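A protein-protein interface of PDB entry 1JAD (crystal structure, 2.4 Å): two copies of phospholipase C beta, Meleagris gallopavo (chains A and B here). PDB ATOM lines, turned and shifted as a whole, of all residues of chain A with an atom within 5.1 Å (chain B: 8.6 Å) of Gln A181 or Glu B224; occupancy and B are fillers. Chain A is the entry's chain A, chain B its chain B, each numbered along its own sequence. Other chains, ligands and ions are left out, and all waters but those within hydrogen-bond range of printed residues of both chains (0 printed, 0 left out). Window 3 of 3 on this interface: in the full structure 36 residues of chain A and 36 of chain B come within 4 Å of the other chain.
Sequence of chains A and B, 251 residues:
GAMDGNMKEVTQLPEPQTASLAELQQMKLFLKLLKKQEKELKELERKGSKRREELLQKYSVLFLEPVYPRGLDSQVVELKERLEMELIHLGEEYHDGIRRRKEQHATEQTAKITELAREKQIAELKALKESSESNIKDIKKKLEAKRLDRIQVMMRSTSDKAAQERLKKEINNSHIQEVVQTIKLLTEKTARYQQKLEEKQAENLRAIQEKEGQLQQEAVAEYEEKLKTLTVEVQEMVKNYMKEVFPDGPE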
ATOM      1  N   GLN A 177      25.489 -19.975  -3.294  1.00  0.00           N
ATOM      2  CA  GLN A 177      26.303 -19.008  -4.027  1.00  0.00           C
ATOM      3  C   GLN A 177      25.763 -18.733  -5.409  1.00  0.00           C
ATOM      4  O   GLN A 177      25.790 -17.606  -5.885  1.00  0.00           O
ATOM      5  CB  GLN A 177      27.755 -19.472  -4.130  1.00  0.00           C
ATOM      6  CG  GLN A 177      28.397 -19.710  -2.783  1.00  0.00           C
ATOM      7  CD  GLN A 177      29.891 -19.551  -2.836  1.00  0.00           C
ATOM      8  OE1 GLN A 177      30.599 -19.833  -1.864  1.00  0.00           O
ATOM      9  NE2 GLN A 177      30.387 -19.072  -3.972  1.00  0.00           N
ATOM     10  N   GLU A 178      25.256 -19.761  -6.060  1.00  0.00           N
ATOM     11  CA  GLU A 178      24.725 -19.533  -7.386  1.00  0.00           C
ATOM     12  C   GLU A 178      23.496 -18.608  -7.356  1.00  0.00           C
ATOM     13  O   GLU A 178      23.310 -17.833  -8.307  1.00  0.00           O
ATOM     14  CB  GLU A 178      24.396 -20.859  -8.068  1.00  0.00           C
ATOM     15  CG  GLU A 178      24.037 -20.696  -9.526  1.00  0.00           C
ATOM     16  CD  GLU A 178      23.913 -22.020 -10.249  1.00  0.00           C
ATOM     17  OE1 GLU A 178      23.622 -22.006 -11.465  1.00  0.00           O
ATOM     18  OE2 GLU A 178      24.106 -23.072  -9.601  1.00  0.00           O
ATOM     19  N   VAL A 179      22.675 -18.654  -6.291  1.00  0.00           N
ATOM     20  CA  VAL A 179      21.508 -17.749  -6.249  1.00  0.00           C
ATOM     21  C   VAL A 179      21.996 -16.321  -6.019  1.00  0.00           C
ATOM     22  O   VAL A 179      21.519 -15.396  -6.657  1.00  0.00           O
ATOM     23  CB  VAL A 179      20.444 -18.080  -5.123  1.00  0.00           C
ATOM     24  CG1 VAL A 179      20.070 -19.547  -5.157  1.00  0.00           C
ATOM     25  CG2 VAL A 179      20.949 -17.654  -3.752  1.00  0.00           C
ATOM     26  N   VAL A 180      22.957 -16.152  -5.115  1.00  0.00           N
ATOM     27  CA  VAL A 180      23.521 -14.836  -4.822  1.00  0.00           C
ATOM     28  C   VAL A 180      24.147 -14.207  -6.061  1.00  0.00           C
ATOM     29  O   VAL A 180      23.878 -13.052  -6.412  1.00  0.00           O
ATOM     30  CB  VAL A 180      24.607 -14.926  -3.708  1.00  0.00           C
ATOM     31  CG1 VAL A 180      25.360 -13.585  -3.575  1.00  0.00           C
ATOM     32  CG2 VAL A 180      23.935 -15.266  -2.383  1.00  0.00           C
ATOM     33  N   GLN A 181      25.005 -14.964  -6.719  1.00  0.00           N
ATOM     34  CA  GLN A 181      25.648 -14.453  -7.917  1.00  0.00           C
ATOM     35  C   GLN A 181      24.623 -14.225  -9.028  1.00  0.00           C
ATOM     36  O   GLN A 181      24.743 -13.267  -9.792  1.00  0.00           O
ATOM     37  CB  GLN A 181      26.737 -15.426  -8.386  1.00  0.00           C
ATOM     38  CG  GLN A 181      27.858 -15.600  -7.386  1.00  0.00           C
ATOM     39  CD  GLN A 181      28.464 -14.281  -6.972  1.00  0.00           C
ATOM     40  OE1 GLN A 181      28.789 -13.450  -7.818  1.00  0.00           O
ATOM     41  NE2 GLN A 181      28.633 -14.081  -5.662  1.00  0.00           N
ATOM     42  N   THR A 182      23.621 -15.096  -9.135  1.00  0.00           N
ATOM     43  CA  THR A 182      22.637 -14.898 -10.192  1.00  0.00           C
ATOM     44  C   THR A 182      21.801 -13.661  -9.882  1.00  0.00           C
ATOM     45  O   THR A 182      21.492 -12.873 -10.775  1.00  0.00           O
ATOM     46  CB  THR A 182      21.725 -16.140 -10.390  1.00  0.00           C
ATOM     47  OG1 THR A 182      21.308 -16.638  -9.118  1.00  0.00           O
ATOM     48  CG2 THR A 182      22.449 -17.242 -11.138  1.00  0.00           C
ATOM     49  N   ILE A 183      21.451 -13.472  -8.615  1.00  0.00           N
ATOM     50  CA  ILE A 183      20.671 -12.298  -8.233  1.00  0.00           C
ATOM     51  C   ILE A 183      21.498 -11.046  -8.449  1.00  0.00           C
ATOM     52  O   ILE A 183      20.972  -9.976  -8.714  1.00  0.00           O
ATOM     53  CB  ILE A 183      20.243 -12.362  -6.762  1.00  0.00           C
ATOM     54  CG1 ILE A 183      19.100 -13.364  -6.602  1.00  0.00           C
ATOM     55  CG2 ILE A 183      19.851 -10.966  -6.267  1.00  0.00           C
ATOM     56  CD1 ILE A 183      18.632 -13.496  -5.167  1.00  0.00           C
ATOM     57  N   LYS A 184      22.809 -11.191  -8.336  1.00  0.00           N
ATOM     58  CA  LYS A 184      23.739 -10.084  -8.527  1.00  0.00           C
ATOM     59  C   LYS A 184      23.801  -9.734 -10.015  1.00  0.00           C
ATOM     60  O   LYS A 184      23.978  -8.571 -10.399  1.00  0.00           O
ATOM     61  CB  LYS A 184      25.105 -10.525  -8.005  1.00  0.00           C
ATOM     62  CG  LYS A 184      26.146  -9.466  -7.913  1.00  0.00           C
ATOM     63  CD  LYS A 184      27.281  -9.986  -7.049  1.00  0.00           C
ATOM     64  CE  LYS A 184      28.369  -8.922  -6.892  1.00  0.00           C
ATOM     65  NZ  LYS A 184      29.489  -9.409  -6.012  1.00  0.00           N
ATOM     66  N   LEU A 185      23.617 -10.750 -10.854  1.00  0.00           N
ATOM     67  CA  LEU A 185      23.642 -10.572 -12.301  1.00  0.00           C
ATOM     68  C   LEU A 185      22.411  -9.823 -12.841  1.00  0.00           C
ATOM     69  O   LEU A 185      22.538  -8.779 -13.482  1.00  0.00           O
ATOM     70  CB  LEU A 185      23.751 -11.938 -12.976  1.00  0.00           C
ATOM     71  CG  LEU A 185      23.758 -11.903 -14.503  1.00  0.00           C
ATOM     72  CD1 LEU A 185      25.010 -11.167 -15.030  1.00  0.00           C
ATOM     73  CD2 LEU A 185      23.705 -13.315 -15.002  1.00  0.00           C
ATOM     74  N   HIS B  95      16.812 -12.228   4.161  1.00  0.00           N
ATOM     75  CA  HIS B  95      17.644 -11.212   3.500  1.00  0.00           C
ATOM     76  C   HIS B  95      17.153 -10.835   2.108  1.00  0.00           C
ATOM     77  O   HIS B  95      17.293  -9.677   1.691  1.00  0.00           O
ATOM     78  CB  HIS B  95      19.100 -11.691   3.466  1.00  0.00           C
ATOM     79  CG  HIS B  95      19.682 -11.932   4.829  1.00  0.00           C
ATOM     80  ND1 HIS B  95      20.027 -10.902   5.685  1.00  0.00           N
ATOM     81  CD2 HIS B  95      19.917 -13.080   5.514  1.00  0.00           C
ATOM     82  CE1 HIS B  95      20.448 -11.400   6.835  1.00  0.00           C
ATOM     83  NE2 HIS B  95      20.391 -12.720   6.758  1.00  0.00           N
ATOM     84  N   ASP B  96      16.571 -11.766   1.362  1.00  0.00           N
ATOM     85  CA  ASP B  96      16.052 -11.343   0.052  1.00  0.00           C
ATOM     86  C   ASP B  96      14.949 -10.281   0.282  1.00  0.00           C
ATOM     87  O   ASP B  96      14.929  -9.215  -0.376  1.00  0.00           O
ATOM     88  CB  ASP B  96      15.499 -12.549  -0.720  1.00  0.00           C
ATOM     89  CG  ASP B  96      15.180 -12.228  -2.174  1.00  0.00           C
ATOM     90  OD1 ASP B  96      15.966 -11.480  -2.809  1.00  0.00           O
ATOM     91  OD2 ASP B  96      14.163 -12.740  -2.703  1.00  0.00           O
ATOM     92  N   ARG B  99      16.160  -7.068   1.094  1.00  0.00           N
ATOM     93  CA  ARG B  99      16.731  -6.636  -0.166  1.00  0.00           C
ATOM     94  C   ARG B  99      15.639  -6.007  -1.025  1.00  0.00           C
ATOM     95  O   ARG B  99      15.789  -4.892  -1.513  1.00  0.00           O
ATOM     96  CB  ARG B  99      17.360  -7.865  -0.844  1.00  0.00           C
ATOM     97  CG  ARG B  99      18.375  -7.610  -1.942  1.00  0.00           C
ATOM     98  CD  ARG B  99      17.758  -7.524  -3.298  1.00  0.00           C
ATOM     99  NE  ARG B  99      16.942  -8.696  -3.594  1.00  0.00           N
ATOM    100  CZ  ARG B  99      16.264  -8.828  -4.731  1.00  0.00           C
ATOM    101  NH1 ARG B  99      16.332  -7.868  -5.643  1.00  0.00           N
ATOM    102  NH2 ARG B  99      15.485  -9.875  -4.938  1.00  0.00           N
ATOM    103  N   GLN B 217      22.192  -0.673  -5.419  1.00  0.00           N
ATOM    104  CA  GLN B 217      23.468  -1.356  -5.326  1.00  0.00           C
ATOM    105  C   GLN B 217      23.796  -1.711  -3.862  1.00  0.00           C
ATOM    106  O   GLN B 217      24.247  -2.822  -3.571  1.00  0.00           O
ATOM    107  CB  GLN B 217      24.534  -0.466  -5.968  1.00  0.00           C
ATOM    108  CG  GLN B 217      25.923  -1.047  -6.005  1.00  0.00           C
ATOM    109  CD  GLN B 217      26.908  -0.119  -6.709  1.00  0.00           C
ATOM    110  OE1 GLN B 217      28.121  -0.360  -6.696  1.00  0.00           O
ATOM    111  NE2 GLN B 217      26.388   0.943  -7.336  1.00  0.00           N
ATOM    112  N   GLU B 218      23.560  -0.797  -2.928  1.00  0.00           N
ATOM    113  CA  GLU B 218      23.821  -1.122  -1.514  1.00  0.00           C
ATOM    114  C   GLU B 218      22.884  -2.235  -1.033  1.00  0.00           C
ATOM    115  O   GLU B 218      23.265  -3.064  -0.204  1.00  0.00           O
ATOM    116  CB  GLU B 218      23.651   0.113  -0.620  1.00  0.00           C
ATOM    117  CG  GLU B 218      24.631   1.254  -0.921  1.00  0.00           C
ATOM    118  CD  GLU B 218      24.301   2.536  -0.173  1.00  0.00           C
ATOM    119  OE1 GLU B 218      24.952   3.577  -0.453  1.00  0.00           O
ATOM    120  OE2 GLU B 218      23.389   2.509   0.697  1.00  0.00           O
ATOM    121  N   ALA B 219      21.663  -2.291  -1.560  1.00  0.00           N
ATOM    122  CA  ALA B 219      20.759  -3.346  -1.109  1.00  0.00           C
ATOM    123  C   ALA B 219      21.276  -4.698  -1.567  1.00  0.00           C
ATOM    124  O   ALA B 219      21.132  -5.689  -0.849  1.00  0.00           O
ATOM    125  CB  ALA B 219      19.344  -3.132  -1.644  1.00  0.00           C
ATOM    126  N   VAL B 220      21.877  -4.763  -2.755  1.00  0.00           N
ATOM    127  CA  VAL B 220      22.353  -6.068  -3.209  1.00  0.00           C
ATOM    128  C   VAL B 220      23.650  -6.491  -2.516  1.00  0.00           C
ATOM    129  O   VAL B 220      23.842  -7.668  -2.241  1.00  0.00           O
ATOM    130  CB  VAL B 220      22.551  -6.124  -4.741  1.00  0.00           C
ATOM    131  CG1 VAL B 220      22.816  -7.573  -5.166  1.00  0.00           C
ATOM    132  CG2 VAL B 220      21.301  -5.617  -5.451  1.00  0.00           C
ATOM    133  N   ALA B 221      24.531  -5.535  -2.231  1.00  0.00           N
ATOM    134  CA  ALA B 221      25.787  -5.852  -1.560  1.00  0.00           C
ATOM    135  C   ALA B 221      25.471  -6.416  -0.186  1.00  0.00           C
ATOM    136  O   ALA B 221      25.946  -7.505   0.181  1.00  0.00           O
ATOM    137  CB  ALA B 221      26.641  -4.603  -1.432  1.00  0.00           C
ATOM    138  N   GLU B 222      24.660  -5.689   0.585  1.00  0.00           N
ATOM    139  CA  GLU B 222      24.287  -6.177   1.910  1.00  0.00           C
ATOM    140  C   GLU B 222      23.736  -7.582   1.781  1.00  0.00           C
ATOM    141  O   GLU B 222      24.130  -8.484   2.532  1.00  0.00           O
ATOM    142  CB  GLU B 222      23.229  -5.300   2.552  1.00  0.00           C
ATOM    143  CG  GLU B 222      22.673  -5.918   3.829  1.00  0.00           C
ATOM    144  CD  GLU B 222      21.651  -5.041   4.513  1.00  0.00           C
ATOM    145  OE1 GLU B 222      20.627  -4.716   3.879  1.00  0.00           O
ATOM    146  OE2 GLU B 222      21.871  -4.680   5.687  1.00  0.00           O
ATOM    147  N   TYR B 223      22.832  -7.776   0.822  1.00  0.00           N
ATOM    148  CA  TYR B 223      22.234  -9.090   0.619  1.00  0.00           C
ATOM    149  C   TYR B 223      23.319 -10.152   0.475  1.00  0.00           C
ATOM    150  O   TYR B 223      23.269 -11.205   1.117  1.00  0.00           O
ATOM    151  CB  TYR B 223      21.351  -9.095  -0.627  1.00  0.00           C
ATOM    152  CG  TYR B 223      20.865 -10.485  -1.000  1.00  0.00           C
ATOM    153  CD1 TYR B 223      19.918 -11.162  -0.215  1.00  0.00           C
ATOM    154  CD2 TYR B 223      21.389 -11.146  -2.117  1.00  0.00           C
ATOM    155  CE1 TYR B 223      19.505 -12.473  -0.543  1.00  0.00           C
ATOM    156  CE2 TYR B 223      20.989 -12.446  -2.452  1.00  0.00           C
ATOM    157  CZ  TYR B 223      20.052 -13.107  -1.671  1.00  0.00           C
ATOM    158  OH  TYR B 223      19.680 -14.397  -2.023  1.00  0.00           O
ATOM    159  N   GLU B 224      24.299  -9.880  -0.380  1.00  0.00           N
ATOM    160  CA  GLU B 224      25.392 -10.818  -0.588  1.00  0.00           C
ATOM    161  C   GLU B 224      26.190 -10.961   0.700  1.00  0.00           C
ATOM    162  O   GLU B 224      26.448 -12.056   1.177  1.00  0.00           O
ATOM    163  CB  GLU B 224      26.303 -10.302  -1.710  1.00  0.00           C
ATOM    164  CG  GLU B 224      27.602 -11.076  -1.882  1.00  0.00           C
ATOM    165  CD  GLU B 224      28.488 -10.522  -3.002  1.00  0.00           C
ATOM    166  OE1 GLU B 224      28.721  -9.293  -3.050  1.00  0.00           O
ATOM    167  OE2 GLU B 224      28.966 -11.321  -3.827  1.00  0.00           O
ATOM    168  N   GLU B 225      26.565  -9.829   1.263  1.00  0.00           N
ATOM    169  CA  GLU B 225      27.353  -9.803   2.483  1.00  0.00           C
ATOM    170  C   GLU B 225      26.716 -10.677   3.568  1.00  0.00           C
ATOM    171  O   GLU B 225      27.419 -11.226   4.416  1.00  0.00           O
ATOM    172  CB  GLU B 225      27.473  -8.355   2.961  1.00  0.00           C
ATOM    173  CG  GLU B 225      28.682  -8.047   3.820  1.00  0.00           C
ATOM    174  CD  GLU B 225      28.783  -8.953   5.018  1.00  0.00           C
ATOM    175  OE1 GLU B 225      27.774  -9.068   5.753  1.00  0.00           O
ATOM    176  OE2 GLU B 225      29.870  -9.547   5.229  1.00  0.00           O
ATOM    177  N   LYS B 226      25.390 -10.821   3.547  1.00  0.00           N
ATOM    178  CA  LYS B 226      24.726 -11.635   4.560  1.00  0.00           C
ATOM    179  C   LYS B 226      24.784 -13.119   4.223  1.00  0.00           C
ATOM    180  O   LYS B 226      25.008 -13.959   5.108  1.00  0.00           O
ATOM    181  CB  LYS B 226      23.255 -11.224   4.725  1.00  0.00           C
ATOM    182  CG  LYS B 226      23.039  -9.775   5.105  1.00  0.00           C
ATOM    183  CD  LYS B 226      23.687  -9.450   6.424  1.00  0.00           C
ATOM    184  CE  LYS B 226      23.596  -7.963   6.705  1.00  0.00           C
ATOM    185  NZ  LYS B 226      24.229  -7.623   8.011  1.00  0.00           N
ATOM    186  N   LEU B 227      24.571 -13.454   2.953  1.00  0.00           N
ATOM    187  CA  LEU B 227      24.595 -14.852   2.566  1.00  0.00           C
ATOM    188  C   LEU B 227      25.984 -15.428   2.602  1.00  0.00           C
ATOM    189  O   LEU B 227      26.158 -16.642   2.575  1.00  0.00           O
ATOM    190  CB  LEU B 227      23.965 -15.054   1.191  1.00  0.00           C
ATOM    191  CG  LEU B 227      22.441 -14.927   1.245  1.00  0.00           C
ATOM    192  CD1 LEU B 227      21.835 -15.334  -0.070  1.00  0.00           C
ATOM    193  CD2 LEU B 227      21.913 -15.845   2.324  1.00  0.00           C
ATOM    194  N   LYS B 228      26.977 -14.553   2.673  1.00  0.00           N
ATOM    195  CA  LYS B 228      28.350 -15.006   2.744  1.00  0.00           C
ATOM    196  C   LYS B 228      28.477 -15.904   3.977  1.00  0.00           C
ATOM    197  O   LYS B 228      28.842 -17.082   3.878  1.00  0.00           O
ATOM    198  CB  LYS B 228      29.300 -13.801   2.861  1.00  0.00           C
ATOM    199  CG  LYS B 228      30.786 -14.148   2.818  1.00  0.00           C
ATOM    200  CD  LYS B 228      31.187 -14.747   1.465  1.00  0.00           C
ATOM    201  CE  LYS B 228      32.687 -15.118   1.393  1.00  0.00           C
ATOM    202  NZ  LYS B 228      33.623 -13.956   1.546  1.00  0.00           N
ATOM    203  N   THR B 229      28.126 -15.349   5.133  1.00  0.00           N
ATOM    204  CA  THR B 229      28.235 -16.065   6.400  1.00  0.00           C
ATOM    205  C   THR B 229      27.017 -16.838   6.892  1.00  0.00           C
ATOM    206  O   THR B 229      27.079 -17.439   7.960  1.00  0.00           O
ATOM    207  CB  THR B 229      28.638 -15.098   7.520  1.00  0.00           C
ATOM    208  OG1 THR B 229      27.660 -14.058   7.626  1.00  0.00           O
ATOM    209  CG2 THR B 229      29.989 -14.468   7.212  1.00  0.00           C
ATOM    210  N   LEU B 230      25.928 -16.849   6.132  1.00  0.00           N
ATOM    211  CA  LEU B 230      24.719 -17.540   6.569  1.00  0.00           C
ATOM    212  C   LEU B 230      24.903 -19.010   6.964  1.00  0.00           C
ATOM    213  O   LEU B 230      24.621 -19.400   8.102  1.00  0.00           O
ATOM    214  CB  LEU B 230      23.635 -17.448   5.489  1.00  0.00           C
ATOM    215  CG  LEU B 230      22.327 -18.172   5.819  1.00  0.00           C
ATOM    216  CD1 LEU B 230      21.591 -17.411   6.914  1.00  0.00           C
ATOM    217  CD2 LEU B 230      21.466 -18.290   4.557  1.00  0.00           C
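Printed residues of chain B that touch a printed residue of chain A: Tyr B223, Glu B224 and Leu B227.
Among the printed residues, Asp or Glu carboxylates within 4 Å of a Lys or Arg side-chain nitrogen of the other chain: Lys A184 with Glu B224 (3.0 Å).
OG1 of Thr A182 sits at hydrogen-bond distance from O of Val A179, 2.8 Å away.
CG2 of Val A179 touches OH of Tyr B223 (3.9 Å).
Val A180 touches Glu B224 (CG1 to CG, 3.8 Å).
Val A180 touches Leu B227.
Ile A183 touches Tyr B223.
OE2 of Glu B224 lies within salt-bridge range of NZ of Lys A184 (3.0 Å).
The side-chain amide nitrogen (NE2) of Gln A181 is in hydrogen-bond range of the side-chain carboxylate (OE2) of Glu B224 (3.3 Å).
Gln A181 touches just one residue of chain B: Glu B224.
Of chain A, only Val A180, Gln A181 and Lys A184 come within 4 Å of Glu B224.
Val A180 touches two residues of chain B.
No residue of chain B comes within 4 Å of Thr A182.
Printed residues of chain B within 4 Å of Ile A183: Tyr B223.
Of the printed residues of chain B, Val A179 touches Tyr B223.
Of the printed residues of chain A, Tyr B223 touches Val A179 (3.9 Å) and Ile A183 (3.4 Å).
Of the printed residues of chain B, Lys A184 touches Glu B224.
Glu B225 touches none of the printed residues of chain A.
The nearest residue of chain B that does not touch Gln A181 is Tyr B223 (6.4 Å).
No position is printed for both chains.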
